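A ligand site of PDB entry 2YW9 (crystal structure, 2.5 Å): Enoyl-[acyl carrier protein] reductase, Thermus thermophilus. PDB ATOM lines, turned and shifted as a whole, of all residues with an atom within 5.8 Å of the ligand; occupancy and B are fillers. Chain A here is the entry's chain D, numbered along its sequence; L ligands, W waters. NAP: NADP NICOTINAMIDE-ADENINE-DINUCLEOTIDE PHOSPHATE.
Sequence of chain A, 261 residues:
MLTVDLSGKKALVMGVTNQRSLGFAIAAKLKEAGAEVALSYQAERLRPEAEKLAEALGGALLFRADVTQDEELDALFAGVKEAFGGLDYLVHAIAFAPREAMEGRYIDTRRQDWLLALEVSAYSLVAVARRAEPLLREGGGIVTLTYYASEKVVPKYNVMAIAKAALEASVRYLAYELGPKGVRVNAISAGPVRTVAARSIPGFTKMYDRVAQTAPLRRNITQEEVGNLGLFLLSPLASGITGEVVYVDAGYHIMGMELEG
NE2 of Gln 42 sits at hydrogen-bond distance from OD1 of Asp 66, at 3.4 Å. The backbone carbonyl oxygen (O) of Leu 145 is in hydrogen-bond range of the side-chain amino group (NZ) of Lys 164. OG of Ser 21 lies within hydrogen-bond range of O of Asn 18, 3.0 Å away. O of Thr 146 is in hydrogen-bond range of N of Ala 190 (3.2 Å). The backbone NH (N) of Thr 146 lies within hydrogen-bond range of the backbone carbonyl oxygen (O) of Ile 188. The backbone NH (N) of Leu 145 is in hydrogen-bond range of the backbone carbonyl oxygen (O) of His 92 (3.4 Å). The backbone carbonyl oxygen (O) of Tyr 41 lies within hydrogen-bond range of the backbone NH (N) of Ala 65, 2.8 Å away. OG1 of Thr 68 is in hydrogen-bond range of OD2 of Asp 66 (2.6 Å).
Water W2 lies within hydrogen-bond range of an oxygen (O2A) of the ligand (2.4 Å), the backbone carbonyl oxygen (O) of Gly 15 (2.5 Å), the backbone NH (N) of Gly 23 (3.0 Å) and the backbone carbonyl oxygen (O) of Ala 93 (3.4 Å). Water W1 lies within hydrogen-bond range of the backbone carbonyl oxygen (O) of His 92 (2.8 Å), an oxygen (O3D) of the ligand (2.9 Å), the backbone NH (N) of Ile 94 (3.1 Å) and the backbone carbonyl oxygen (O) of Leu 145 (3.4 Å). Water W3 lies within hydrogen-bond range of N of Gly 15 (3.2 Å), N3A of the ligand (3.3 Å) and N of Gln 42 (3.4 Å).
OG1 of Thr 17 sits at hydrogen-bond distance from O1A of the ligand (2.8 Å). N of Leu 22 lies within hydrogen-bond range of O2N of the ligand (2.8 Å). An oxygen (O3X) of the ligand sits close to the side-chain amide oxygen of Gln 42, 2.9 Å away. N of Val 193 sits at hydrogen-bond distance from O7N of the ligand. O2D of the ligand lies within hydrogen-bond range of NZ of Lys 164. N of Val 67 lies within hydrogen-bond range of N1A of the ligand. The side-chain hydroxyl (OG) of Ser 21 sits at hydrogen-bond distance from an oxygen (O2A) of the ligand, at 3.2 Å. O3B of the ligand lies within hydrogen-bond range of N of Val 16 (3.3 Å).
Residues that only touch the ligand: Gly 15, Leu 46, Ala 65, Asp 66, Thr 68, Ala 93, Ile 94, Ala 95, Phe 96, Val 120, Leu 145, Thr 146, Tyr 147, Tyr 157, Met 160, Ala 190, Gly 191, Pro 192 and Phe 204. Hydrophobic or aromatic side chains within 4 Å of the ligand: Leu 22, Leu 46, Val 67, Ile 94, Ala 95, Phe 96, Val 120, Leu 145, Tyr 147, Met 160, Ala 190 and Phe 204. The nearest printed residue that does not touch the ligand is Gly 23 (4.5 Å).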
ATOM      1  N   GLY A  15       4.486  20.390  -6.600  1.00  0.00           N
ATOM      2  CA  GLY A  15       3.103  19.965  -6.824  1.00  0.00           C
ATOM      3  C   GLY A  15       2.229  21.066  -7.368  1.00  0.00           C
ATOM      4  O   GLY A  15       1.348  21.568  -6.681  1.00  0.00           O
ATOM      5  N   VAL A  16       2.473  21.449  -8.610  1.00  0.00           N
ATOM      6  CA  VAL A  16       1.729  22.530  -9.239  1.00  0.00           C
ATOM      7  C   VAL A  16       1.235  22.097 -10.640  1.00  0.00           C
ATOM      8  O   VAL A  16       2.004  21.584 -11.448  1.00  0.00           O
ATOM      9  CB  VAL A  16       2.598  23.801  -9.308  1.00  0.00           C
ATOM     10  CG1 VAL A  16       2.560  24.446 -10.682  1.00  0.00           C
ATOM     11  CG2 VAL A  16       2.213  24.766  -8.206  1.00  0.00           C
ATOM     12  N   THR A  17      -0.062  22.270 -10.886  1.00  0.00           N
ATOM     13  CA  THR A  17      -0.596  21.958 -12.216  1.00  0.00           C
ATOM     14  C   THR A  17      -1.473  23.056 -12.790  1.00  0.00           C
ATOM     15  O   THR A  17      -1.348  23.392 -13.967  1.00  0.00           O
ATOM     16  CB  THR A  17      -1.321  20.588 -12.278  1.00  0.00           C
ATOM     17  OG1 THR A  17      -1.815  20.218 -10.987  1.00  0.00           O
ATOM     18  CG2 THR A  17      -0.377  19.531 -12.731  1.00  0.00           C
ATOM     19  N   ASN A  18      -2.349  23.612 -11.962  1.00  0.00           N
ATOM     20  CA  ASN A  18      -3.198  24.731 -12.380  1.00  0.00           C
ATOM     21  C   ASN A  18      -3.172  25.867 -11.372  1.00  0.00           C
ATOM     22  O   ASN A  18      -2.607  25.731 -10.288  1.00  0.00           O
ATOM     23  CB  ASN A  18      -4.648  24.258 -12.617  1.00  0.00           C
ATOM     24  N   ARG A  20      -5.579  26.758  -9.749  1.00  0.00           N
ATOM     25  CA  ARG A  20      -6.501  26.358  -8.704  1.00  0.00           C
ATOM     26  C   ARG A  20      -5.881  25.338  -7.740  1.00  0.00           C
ATOM     27  O   ARG A  20      -6.544  24.838  -6.837  1.00  0.00           O
ATOM     28  CB  ARG A  20      -7.810  25.827  -9.315  1.00  0.00           C
ATOM     29  N   SER A  21      -4.603  25.034  -7.944  1.00  0.00           N
ATOM     30  CA  SER A  21      -3.870  24.140  -7.031  1.00  0.00           C
ATOM     31  C   SER A  21      -3.621  24.784  -5.678  1.00  0.00           C
ATOM     32  O   SER A  21      -3.228  25.956  -5.606  1.00  0.00           O
ATOM     33  CB  SER A  21      -2.501  23.779  -7.604  1.00  0.00           C
ATOM     34  OG  SER A  21      -2.604  23.119  -8.835  1.00  0.00           O
ATOM     35  N   LEU A  22      -3.799  24.013  -4.621  1.00  0.00           N
ATOM     36  CA  LEU A  22      -3.507  24.497  -3.277  1.00  0.00           C
ATOM     37  C   LEU A  22      -2.035  24.885  -3.134  1.00  0.00           C
ATOM     38  O   LEU A  22      -1.697  25.808  -2.392  1.00  0.00           O
ATOM     39  CB  LEU A  22      -3.881  23.455  -2.220  1.00  0.00           C
ATOM     40  CG  LEU A  22      -5.335  22.974  -2.220  1.00  0.00           C
ATOM     41  CD1 LEU A  22      -5.608  22.190  -0.952  1.00  0.00           C
ATOM     42  CD2 LEU A  22      -6.330  24.138  -2.362  1.00  0.00           C
ATOM     43  N   GLY A  23      -1.166  24.166  -3.839  1.00  0.00           N
ATOM     44  CA  GLY A  23       0.262  24.484  -3.871  1.00  0.00           C
ATOM     45  C   GLY A  23       0.513  25.875  -4.426  1.00  0.00           C
ATOM     46  O   GLY A  23       1.302  26.642  -3.866  1.00  0.00           O
ATOM     47  N   TYR A  41       7.316  21.022 -11.440  1.00  0.00           N
ATOM     48  CA  TYR A  41       6.230  20.350 -12.144  1.00  0.00           C
ATOM     49  C   TYR A  41       6.597  18.889 -12.366  1.00  0.00           C
ATOM     50  O   TYR A  41       7.777  18.527 -12.391  1.00  0.00           O
ATOM     51  CB  TYR A  41       5.961  21.040 -13.494  1.00  0.00           C
ATOM     52  N   GLN A  42       5.576  18.041 -12.555  1.00  0.00           N
ATOM     53  CA  GLN A  42       5.796  16.600 -12.665  1.00  0.00           C
ATOM     54  C   GLN A  42       6.451  16.172 -13.994  1.00  0.00           C
ATOM     55  O   GLN A  42       7.499  15.531 -13.992  1.00  0.00           O
ATOM     56  CB  GLN A  42       4.480  15.836 -12.463  1.00  0.00           C
ATOM     57  CG  GLN A  42       4.596  14.320 -12.586  1.00  0.00           C
ATOM     58  CD  GLN A  42       3.283  13.610 -12.348  1.00  0.00           C
ATOM     59  OE1 GLN A  42       2.283  14.225 -11.994  1.00  0.00           O
ATOM     60  NE2 GLN A  42       3.276  12.297 -12.540  1.00  0.00           N
ATOM     61  N   ALA A  43       5.822  16.540 -15.107  1.00  0.00           N
ATOM     62  CA  ALA A  43       6.274  16.111 -16.424  1.00  0.00           C
ATOM     63  C   ALA A  43       6.149  17.210 -17.486  1.00  0.00           C
ATOM     64  O   ALA A  43       5.550  18.263 -17.242  1.00  0.00           O
ATOM     65  CB  ALA A  43       5.524  14.852 -16.870  1.00  0.00           C
ATOM     66  N   LEU A  46       3.100  19.637 -18.611  1.00  0.00           N
ATOM     67  CA  LEU A  46       2.608  20.759 -17.803  1.00  0.00           C
ATOM     68  C   LEU A  46       3.514  21.988 -17.787  1.00  0.00           C
ATOM     69  O   LEU A  46       3.168  23.013 -17.185  1.00  0.00           O
ATOM     70  CB  LEU A  46       2.360  20.296 -16.365  1.00  0.00           C
ATOM     71  CG  LEU A  46       1.465  19.072 -16.218  1.00  0.00           C
ATOM     72  CD1 LEU A  46       1.800  18.327 -14.934  1.00  0.00           C
ATOM     73  CD2 LEU A  46      -0.017  19.458 -16.279  1.00  0.00           C
ATOM     74  N   ALA A  65      10.369  17.555 -11.879  1.00  0.00           N
ATOM     75  CA  ALA A  65      10.755  16.480 -10.985  1.00  0.00           C
ATOM     76  C   ALA A  65       9.583  15.536 -10.779  1.00  0.00           C
ATOM     77  O   ALA A  65       8.477  15.953 -10.411  1.00  0.00           O
ATOM     78  CB  ALA A  65      11.261  17.018  -9.649  1.00  0.00           C
ATOM     79  N   ASP A  66       9.836  14.258 -11.033  1.00  0.00           N
ATOM     80  CA  ASP A  66       8.896  13.202 -10.697  1.00  0.00           C
ATOM     81  C   ASP A  66       9.379  12.562  -9.409  1.00  0.00           C
ATOM     82  O   ASP A  66      10.534  12.129  -9.314  1.00  0.00           O
ATOM     83  CB  ASP A  66       8.809  12.176 -11.819  1.00  0.00           C
ATOM     84  CG  ASP A  66       7.629  11.243 -11.654  1.00  0.00           C
ATOM     85  OD1 ASP A  66       6.576  11.498 -12.273  1.00  0.00           O
ATOM     86  OD2 ASP A  66       7.751  10.261 -10.881  1.00  0.00           O
ATOM     87  N   VAL A  67       8.500  12.509  -8.414  1.00  0.00           N
ATOM     88  CA  VAL A  67       8.901  12.115  -7.073  1.00  0.00           C
ATOM     89  C   VAL A  67       9.157  10.616  -6.938  1.00  0.00           C
ATOM     90  O   VAL A  67       9.716  10.168  -5.943  1.00  0.00           O
ATOM     91  CB  VAL A  67       7.898  12.583  -6.011  1.00  0.00           C
ATOM     92  CG1 VAL A  67       7.851  14.107  -5.990  1.00  0.00           C
ATOM     93  CG2 VAL A  67       6.517  12.000  -6.269  1.00  0.00           C
ATOM     94  N   THR A  68       8.764   9.838  -7.944  1.00  0.00           N
ATOM     95  CA  THR A  68       9.062   8.419  -7.953  1.00  0.00           C
ATOM     96  C   THR A  68      10.499   8.148  -8.405  1.00  0.00           C
ATOM     97  O   THR A  68      11.020   7.060  -8.216  1.00  0.00           O
ATOM     98  CB  THR A  68       8.071   7.611  -8.862  1.00  0.00           C
ATOM     99  OG1 THR A  68       8.395   7.804 -10.239  1.00  0.00           O
ATOM    100  CG2 THR A  68       6.647   8.055  -8.628  1.00  0.00           C
ATOM    101  N   HIS A  92       5.180  20.913   0.258  1.00  0.00           N
ATOM    102  CA  HIS A  92       4.886  19.615  -0.295  1.00  0.00           C
ATOM    103  C   HIS A  92       3.390  19.491  -0.631  1.00  0.00           C
ATOM    104  O   HIS A  92       2.564  19.217   0.248  1.00  0.00           O
ATOM    105  CB  HIS A  92       5.321  18.543   0.686  1.00  0.00           C
ATOM    106  CG  HIS A  92       5.120  17.147   0.184  1.00  0.00           C
ATOM    107  ND1 HIS A  92       4.025  16.389   0.543  1.00  0.00           N
ATOM    108  CD2 HIS A  92       5.876  16.365  -0.612  1.00  0.00           C
ATOM    109  CE1 HIS A  92       4.106  15.205  -0.038  1.00  0.00           C
ATOM    110  NE2 HIS A  92       5.226  15.161  -0.735  1.00  0.00           N
ATOM    111  N   ALA A  93       3.060  19.694  -1.896  1.00  0.00           N
ATOM    112  CA  ALA A  93       1.661  19.666  -2.332  1.00  0.00           C
ATOM    113  C   ALA A  93       1.460  18.596  -3.397  1.00  0.00           C
ATOM    114  O   ALA A  93       0.905  18.861  -4.448  1.00  0.00           O
ATOM    115  CB  ALA A  93       1.248  21.032  -2.873  1.00  0.00           C
ATOM    116  N   ILE A  94       1.942  17.388  -3.104  1.00  0.00           N
ATOM    117  CA  ILE A  94       1.884  16.280  -4.046  1.00  0.00           C
ATOM    118  C   ILE A  94       1.048  15.124  -3.497  1.00  0.00           C
ATOM    119  O   ILE A  94       1.208  14.722  -2.353  1.00  0.00           O
ATOM    120  CB  ILE A  94       3.299  15.786  -4.396  1.00  0.00           C
ATOM    121  CG1 ILE A  94       4.028  16.857  -5.206  1.00  0.00           C
ATOM    122  CG2 ILE A  94       3.244  14.468  -5.162  1.00  0.00           C
ATOM    123  CD1 ILE A  94       5.490  16.604  -5.389  1.00  0.00           C
ATOM    124  N   ALA A  95       0.121  14.634  -4.313  1.00  0.00           N
ATOM    125  CA  ALA A  95      -0.687  13.469  -3.967  1.00  0.00           C
ATOM    126  C   ALA A  95      -1.111  12.777  -5.242  1.00  0.00           C
ATOM    127  O   ALA A  95      -1.320  13.422  -6.273  1.00  0.00           O
ATOM    128  CB  ALA A  95      -1.897  13.872  -3.177  1.00  0.00           C
ATOM    129  N   PHE A  96      -1.227  11.448  -5.184  1.00  0.00           N
ATOM    130  CA  PHE A  96      -1.689  10.662  -6.305  1.00  0.00           C
ATOM    131  C   PHE A  96      -2.088   9.265  -5.869  1.00  0.00           C
ATOM    132  O   PHE A  96      -1.413   8.641  -5.043  1.00  0.00           O
ATOM    133  CB  PHE A  96      -0.621  10.560  -7.396  1.00  0.00           C
ATOM    134  CG  PHE A  96      -1.000   9.667  -8.540  1.00  0.00           C
ATOM    135  CD1 PHE A  96      -1.873  10.122  -9.533  1.00  0.00           C
ATOM    136  CD2 PHE A  96      -0.500   8.377  -8.639  1.00  0.00           C
ATOM    137  CE1 PHE A  96      -2.239   9.302 -10.601  1.00  0.00           C
ATOM    138  CE2 PHE A  96      -0.857   7.548  -9.704  1.00  0.00           C
ATOM    139  CZ  PHE A  96      -1.724   8.012 -10.689  1.00  0.00           C
ATOM    140  N   VAL A 120       3.957   7.913  -3.740  1.00  0.00           N
ATOM    141  CA  VAL A 120       3.864   9.280  -4.236  1.00  0.00           C
ATOM    142  C   VAL A 120       3.358  10.213  -3.155  1.00  0.00           C
ATOM    143  O   VAL A 120       3.883  11.320  -2.978  1.00  0.00           O
ATOM    144  CB  VAL A 120       2.916   9.344  -5.475  1.00  0.00           C
ATOM    145  CG1 VAL A 120       2.689  10.779  -5.910  1.00  0.00           C
ATOM    146  CG2 VAL A 120       3.471   8.521  -6.619  1.00  0.00           C
ATOM    147  N   LEU A 145       0.258  18.797   2.717  1.00  0.00           N
ATOM    148  CA  LEU A 145      -1.201  18.919   2.671  1.00  0.00           C
ATOM    149  C   LEU A 145      -1.881  17.574   2.830  1.00  0.00           C
ATOM    150  O   LEU A 145      -1.498  16.596   2.196  1.00  0.00           O
ATOM    151  CB  LEU A 145      -1.631  19.573   1.361  1.00  0.00           C
ATOM    152  CG  LEU A 145      -1.371  21.086   1.284  1.00  0.00           C
ATOM    153  CD1 LEU A 145      -0.795  21.441  -0.059  1.00  0.00           C
ATOM    154  CD2 LEU A 145      -2.635  21.876   1.561  1.00  0.00           C
ATOM    155  N   THR A 146      -2.896  17.543   3.687  1.00  0.00           N
ATOM    156  CA  THR A 146      -3.602  16.317   4.002  1.00  0.00           C
ATOM    157  C   THR A 146      -5.100  16.570   4.096  1.00  0.00           C
ATOM    158  O   THR A 146      -5.573  17.670   3.818  1.00  0.00           O
ATOM    159  CB  THR A 146      -3.085  15.706   5.313  1.00  0.00           C
ATOM    160  OG1 THR A 146      -3.646  14.403   5.495  1.00  0.00           O
ATOM    161  CG2 THR A 146      -3.436  16.608   6.503  1.00  0.00           C
ATOM    162  N   TYR A 147      -5.845  15.543   4.503  1.00  0.00           N
ATOM    163  CA  TYR A 147      -7.313  15.618   4.573  1.00  0.00           C
ATOM    164  C   TYR A 147      -7.845  14.719   5.679  1.00  0.00           C
ATOM    165  O   TYR A 147      -7.231  13.703   6.024  1.00  0.00           O
ATOM    166  CB  TYR A 147      -7.923  15.253   3.208  1.00  0.00           C
ATOM    167  CG  TYR A 147      -9.427  15.231   3.163  1.00  0.00           C
ATOM    168  CD1 TYR A 147     -10.162  16.413   3.298  1.00  0.00           C
ATOM    169  CD2 TYR A 147     -10.119  14.040   2.976  1.00  0.00           C
ATOM    170  CE1 TYR A 147     -11.550  16.395   3.259  1.00  0.00           C
ATOM    171  CE2 TYR A 147     -11.500  14.016   2.927  1.00  0.00           C
ATOM    172  CZ  TYR A 147     -12.209  15.187   3.076  1.00  0.00           C
ATOM    173  OH  TYR A 147     -13.590  15.163   3.027  1.00  0.00           O
ATOM    174  N   TYR A 157     -12.610   7.846  -0.757  1.00  0.00           N
ATOM    175  CA  TYR A 157     -11.262   8.411  -0.631  1.00  0.00           C
ATOM    176  C   TYR A 157     -10.231   7.272  -0.556  1.00  0.00           C
ATOM    177  O   TYR A 157      -9.047   7.479  -0.790  1.00  0.00           O
ATOM    178  CB  TYR A 157     -11.161   9.363   0.573  1.00  0.00           C
ATOM    179  CG  TYR A 157     -10.139  10.474   0.407  1.00  0.00           C
ATOM    180  CD1 TYR A 157     -10.388  11.579  -0.418  1.00  0.00           C
ATOM    181  CD2 TYR A 157      -8.921  10.435   1.087  1.00  0.00           C
ATOM    182  CE1 TYR A 157      -9.448  12.608  -0.560  1.00  0.00           C
ATOM    183  CE2 TYR A 157      -7.972  11.453   0.948  1.00  0.00           C
ATOM    184  CZ  TYR A 157      -8.240  12.537   0.114  1.00  0.00           C
ATOM    185  OH  TYR A 157      -7.294  13.544  -0.020  1.00  0.00           O
ATOM    186  N   MET A 160      -6.103   6.787  -0.523  1.00  0.00           N
ATOM    187  CA  MET A 160      -5.578   8.120  -0.256  1.00  0.00           C
ATOM    188  C   MET A 160      -5.694   8.486   1.218  1.00  0.00           C
ATOM    189  O   MET A 160      -4.818   9.133   1.766  1.00  0.00           O
ATOM    190  CB  MET A 160      -6.275   9.157  -1.139  1.00  0.00           C
ATOM    191  CG  MET A 160      -5.504   9.457  -2.418  1.00  0.00           C
ATOM    192  SD  MET A 160      -3.964  10.310  -2.031  1.00  0.00           S
ATOM    193  CE  MET A 160      -4.612  11.878  -1.489  1.00  0.00           C
ATOM    194  N   LYS A 164      -2.608   9.506   3.481  1.00  0.00           N
ATOM    195  CA  LYS A 164      -2.627  10.679   4.344  1.00  0.00           C
ATOM    196  C   LYS A 164      -2.329  10.303   5.786  1.00  0.00           C
ATOM    197  O   LYS A 164      -1.666  11.059   6.498  1.00  0.00           O
ATOM    198  CB  LYS A 164      -3.972  11.389   4.251  1.00  0.00           C
ATOM    199  CG  LYS A 164      -4.259  12.006   2.885  1.00  0.00           C
ATOM    200  CD  LYS A 164      -3.062  12.776   2.359  1.00  0.00           C
ATOM    201  CE  LYS A 164      -3.449  13.604   1.160  1.00  0.00           C
ATOM    202  NZ  LYS A 164      -2.342  14.502   0.725  1.00  0.00           N
ATOM    203  N   ILE A 188      -1.157  20.913   6.609  1.00  0.00           N
ATOM    204  CA  ILE A 188      -2.413  21.642   6.457  1.00  0.00           C
ATOM    205  C   ILE A 188      -3.486  20.643   6.082  1.00  0.00           C
ATOM    206  O   ILE A 188      -3.400  19.996   5.039  1.00  0.00           O
ATOM    207  CB  ILE A 188      -2.300  22.706   5.343  1.00  0.00           C
ATOM    208  CG1 ILE A 188      -1.291  23.787   5.731  1.00  0.00           C
ATOM    209  CG2 ILE A 188      -3.648  23.338   5.051  1.00  0.00           C
ATOM    210  CD1 ILE A 188      -0.886  24.661   4.579  1.00  0.00           C
ATOM    211  N   SER A 189      -4.491  20.479   6.931  1.00  0.00           N
ATOM    212  CA  SER A 189      -5.619  19.618   6.560  1.00  0.00           C
ATOM    213  C   SER A 189      -6.718  20.458   5.934  1.00  0.00           C
ATOM    214  O   SER A 189      -7.555  21.005   6.631  1.00  0.00           O
ATOM    215  CB  SER A 189      -6.153  18.855   7.769  1.00  0.00           C
ATOM    216  OG  SER A 189      -6.865  17.721   7.348  1.00  0.00           O
ATOM    217  N   ALA A 190      -6.699  20.580   4.610  1.00  0.00           N
ATOM    218  CA  ALA A 190      -7.675  21.398   3.908  1.00  0.00           C
ATOM    219  C   ALA A 190      -8.997  20.673   3.763  1.00  0.00           C
ATOM    220  O   ALA A 190      -9.027  19.445   3.703  1.00  0.00           O
ATOM    221  CB  ALA A 190      -7.140  21.787   2.538  1.00  0.00           C
ATOM    222  N   GLY A 191     -10.082  21.437   3.719  1.00  0.00           N
ATOM    223  CA  GLY A 191     -11.376  20.914   3.301  1.00  0.00           C
ATOM    224  C   GLY A 191     -11.394  20.868   1.784  1.00  0.00           C
ATOM    225  O   GLY A 191     -10.457  21.332   1.133  1.00  0.00           O
ATOM    226  N   PRO A 192     -12.460  20.310   1.203  1.00  0.00           N
ATOM    227  CA  PRO A 192     -12.581  20.251  -0.251  1.00  0.00           C
ATOM    228  C   PRO A 192     -12.616  21.625  -0.923  1.00  0.00           C
ATOM    229  O   PRO A 192     -13.323  22.514  -0.461  1.00  0.00           O
ATOM    230  CB  PRO A 192     -13.907  19.519  -0.479  1.00  0.00           C
ATOM    231  CG  PRO A 192     -14.644  19.613   0.801  1.00  0.00           C
ATOM    232  CD  PRO A 192     -13.606  19.671   1.881  1.00  0.00           C
ATOM    233  N   VAL A 193     -11.824  21.777  -1.977  1.00  0.00           N
ATOM    234  CA  VAL A 193     -11.799  22.990  -2.786  1.00  0.00           C
ATOM    235  C   VAL A 193     -12.036  22.646  -4.255  1.00  0.00           C
ATOM    236  O   VAL A 193     -11.441  21.684  -4.772  1.00  0.00           O
ATOM    237  CB  VAL A 193     -10.455  23.733  -2.656  1.00  0.00           C
ATOM    238  CG1 VAL A 193     -10.400  24.907  -3.639  1.00  0.00           C
ATOM    239  CG2 VAL A 193     -10.239  24.225  -1.233  1.00  0.00           C
ATOM    240  N   PHE A 204     -16.488  13.638  -5.664  1.00  0.00           N
ATOM    241  CA  PHE A 204     -16.046  14.882  -5.030  1.00  0.00           C
ATOM    242  C   PHE A 204     -17.177  15.834  -4.632  1.00  0.00           C
ATOM    243  O   PHE A 204     -17.225  16.296  -3.482  1.00  0.00           O
ATOM    244  CB  PHE A 204     -15.035  15.619  -5.929  1.00  0.00           C
ATOM    245  CG  PHE A 204     -14.519  16.904  -5.329  1.00  0.00           C
ATOM    246  CD1 PHE A 204     -13.515  16.887  -4.366  1.00  0.00           C
ATOM    247  CD2 PHE A 204     -15.042  18.135  -5.718  1.00  0.00           C
ATOM    248  CE1 PHE A 204     -13.046  18.065  -3.815  1.00  0.00           C
ATOM    249  CE2 PHE A 204     -14.567  19.316  -5.175  1.00  0.00           C
ATOM    250  CZ  PHE A 204     -13.574  19.277  -4.215  1.00  0.00           C
HETATM  251  PA  NAP L   1      -3.224  19.453  -7.568  1.00  0.00           P
HETATM  252  O1A NAP L   1      -3.631  19.773  -8.943  1.00  0.00           O
HETATM  253  O2A NAP L   1      -2.288  20.488  -7.094  1.00  0.00           O
HETATM  254  O5B NAP L   1      -2.543  17.979  -7.524  1.00  0.00           O
HETATM  255  C5B NAP L   1      -1.435  17.656  -6.687  1.00  0.00           C
HETATM  256  C4B NAP L   1      -0.109  17.785  -7.442  1.00  0.00           C
HETATM  257  O4B NAP L   1       0.728  16.655  -7.242  1.00  0.00           O
HETATM  258  C3B NAP L   1      -0.319  17.918  -8.946  1.00  0.00           C
HETATM  259  O3B NAP L   1       0.413  19.021  -9.434  1.00  0.00           O
HETATM  260  C2B NAP L   1       0.275  16.637  -9.488  1.00  0.00           C
HETATM  261  O2B NAP L   1       0.703  16.730 -10.832  1.00  0.00           O
HETATM  262  C1B NAP L   1       1.361  16.344  -8.475  1.00  0.00           C
HETATM  263  N9A NAP L   1       1.820  14.950  -8.631  1.00  0.00           N
HETATM  264  C8A NAP L   1       1.077  13.796  -8.684  1.00  0.00           C
HETATM  265  N7A NAP L   1       1.910  12.747  -8.865  1.00  0.00           N
HETATM  266  C5A NAP L   1       3.190  13.202  -8.933  1.00  0.00           C
HETATM  267  C6A NAP L   1       4.418  12.576  -9.107  1.00  0.00           C
HETATM  268  N6A NAP L   1       4.503  11.258  -9.238  1.00  0.00           N
HETATM  269  N1A NAP L   1       5.567  13.337  -9.132  1.00  0.00           N
HETATM  270  C2A NAP L   1       5.505  14.698  -8.995  1.00  0.00           C
HETATM  271  N3A NAP L   1       4.278  15.315  -8.824  1.00  0.00           N
HETATM  272  C4A NAP L   1       3.139  14.585  -8.792  1.00  0.00           C
HETATM  273  O3  NAP L   1      -4.522  19.360  -6.600  1.00  0.00           O
HETATM  274  PN  NAP L   1      -4.718  19.820  -5.054  1.00  0.00           P
HETATM  275  O1N NAP L   1      -6.041  19.338  -4.565  1.00  0.00           O
HETATM  276  O2N NAP L   1      -4.348  21.244  -4.923  1.00  0.00           O
HETATM  277  O5D NAP L   1      -3.566  18.937  -4.331  1.00  0.00           O
HETATM  278  C5D NAP L   1      -2.610  19.519  -3.459  1.00  0.00           C
HETATM  279  C4D NAP L   1      -2.608  18.756  -2.132  1.00  0.00           C
HETATM  280  O4D NAP L   1      -3.709  19.139  -1.325  1.00  0.00           O
HETATM  281  C3D NAP L   1      -2.743  17.253  -2.348  1.00  0.00           C
HETATM  282  O3D NAP L   1      -1.800  16.596  -1.528  1.00  0.00           O
HETATM  283  C2D NAP L   1      -4.148  16.932  -1.904  1.00  0.00           C
HETATM  284  O2D NAP L   1      -4.264  15.622  -1.415  1.00  0.00           O
HETATM  285  C1D NAP L   1      -4.374  17.992  -0.833  1.00  0.00           C
HETATM  286  N1N NAP L   1      -5.807  18.297  -0.597  1.00  0.00           N
HETATM  287  C2N NAP L   1      -6.595  18.724  -1.631  1.00  0.00           C
HETATM  288  C3N NAP L   1      -7.934  19.015  -1.411  1.00  0.00           C
HETATM  289  C7N NAP L   1      -8.799  19.486  -2.558  1.00  0.00           C
HETATM  290  O7N NAP L   1     -10.197  19.380  -2.447  1.00  0.00           O
HETATM  291  N7N NAP L   1      -8.234  20.003  -3.638  1.00  0.00           N
HETATM  292  C4N NAP L   1      -8.461  18.878  -0.140  1.00  0.00           C
HETATM  293  C5N NAP L   1      -7.650  18.444   0.894  1.00  0.00           C
HETATM  294  C6N NAP L   1      -6.314  18.156   0.661  1.00  0.00           C
HETATM  295  P2B NAP L   1      -0.274  16.084 -11.963  1.00  0.00           P
HETATM  296  O1X NAP L   1      -1.603  16.814 -11.972  1.00  0.00           O
HETATM  297  O2X NAP L   1       0.382  16.192 -13.321  1.00  0.00           O
HETATM  298  O3X NAP L   1      -0.537  14.620 -11.663  1.00  0.00           O
HETATM  299  O   HOH W   1       0.774  17.074  -0.273  1.00  0.00           O
HETATM  300  O   HOH W   2      -0.855  21.610  -5.470  1.00  0.00           O
HETATM  301  O   HOH W   3       4.865  18.517  -9.221  1.00  0.00           O
HETATM  302  O   HOH W   4      -7.427  21.095  -6.745  1.00  0.00           O
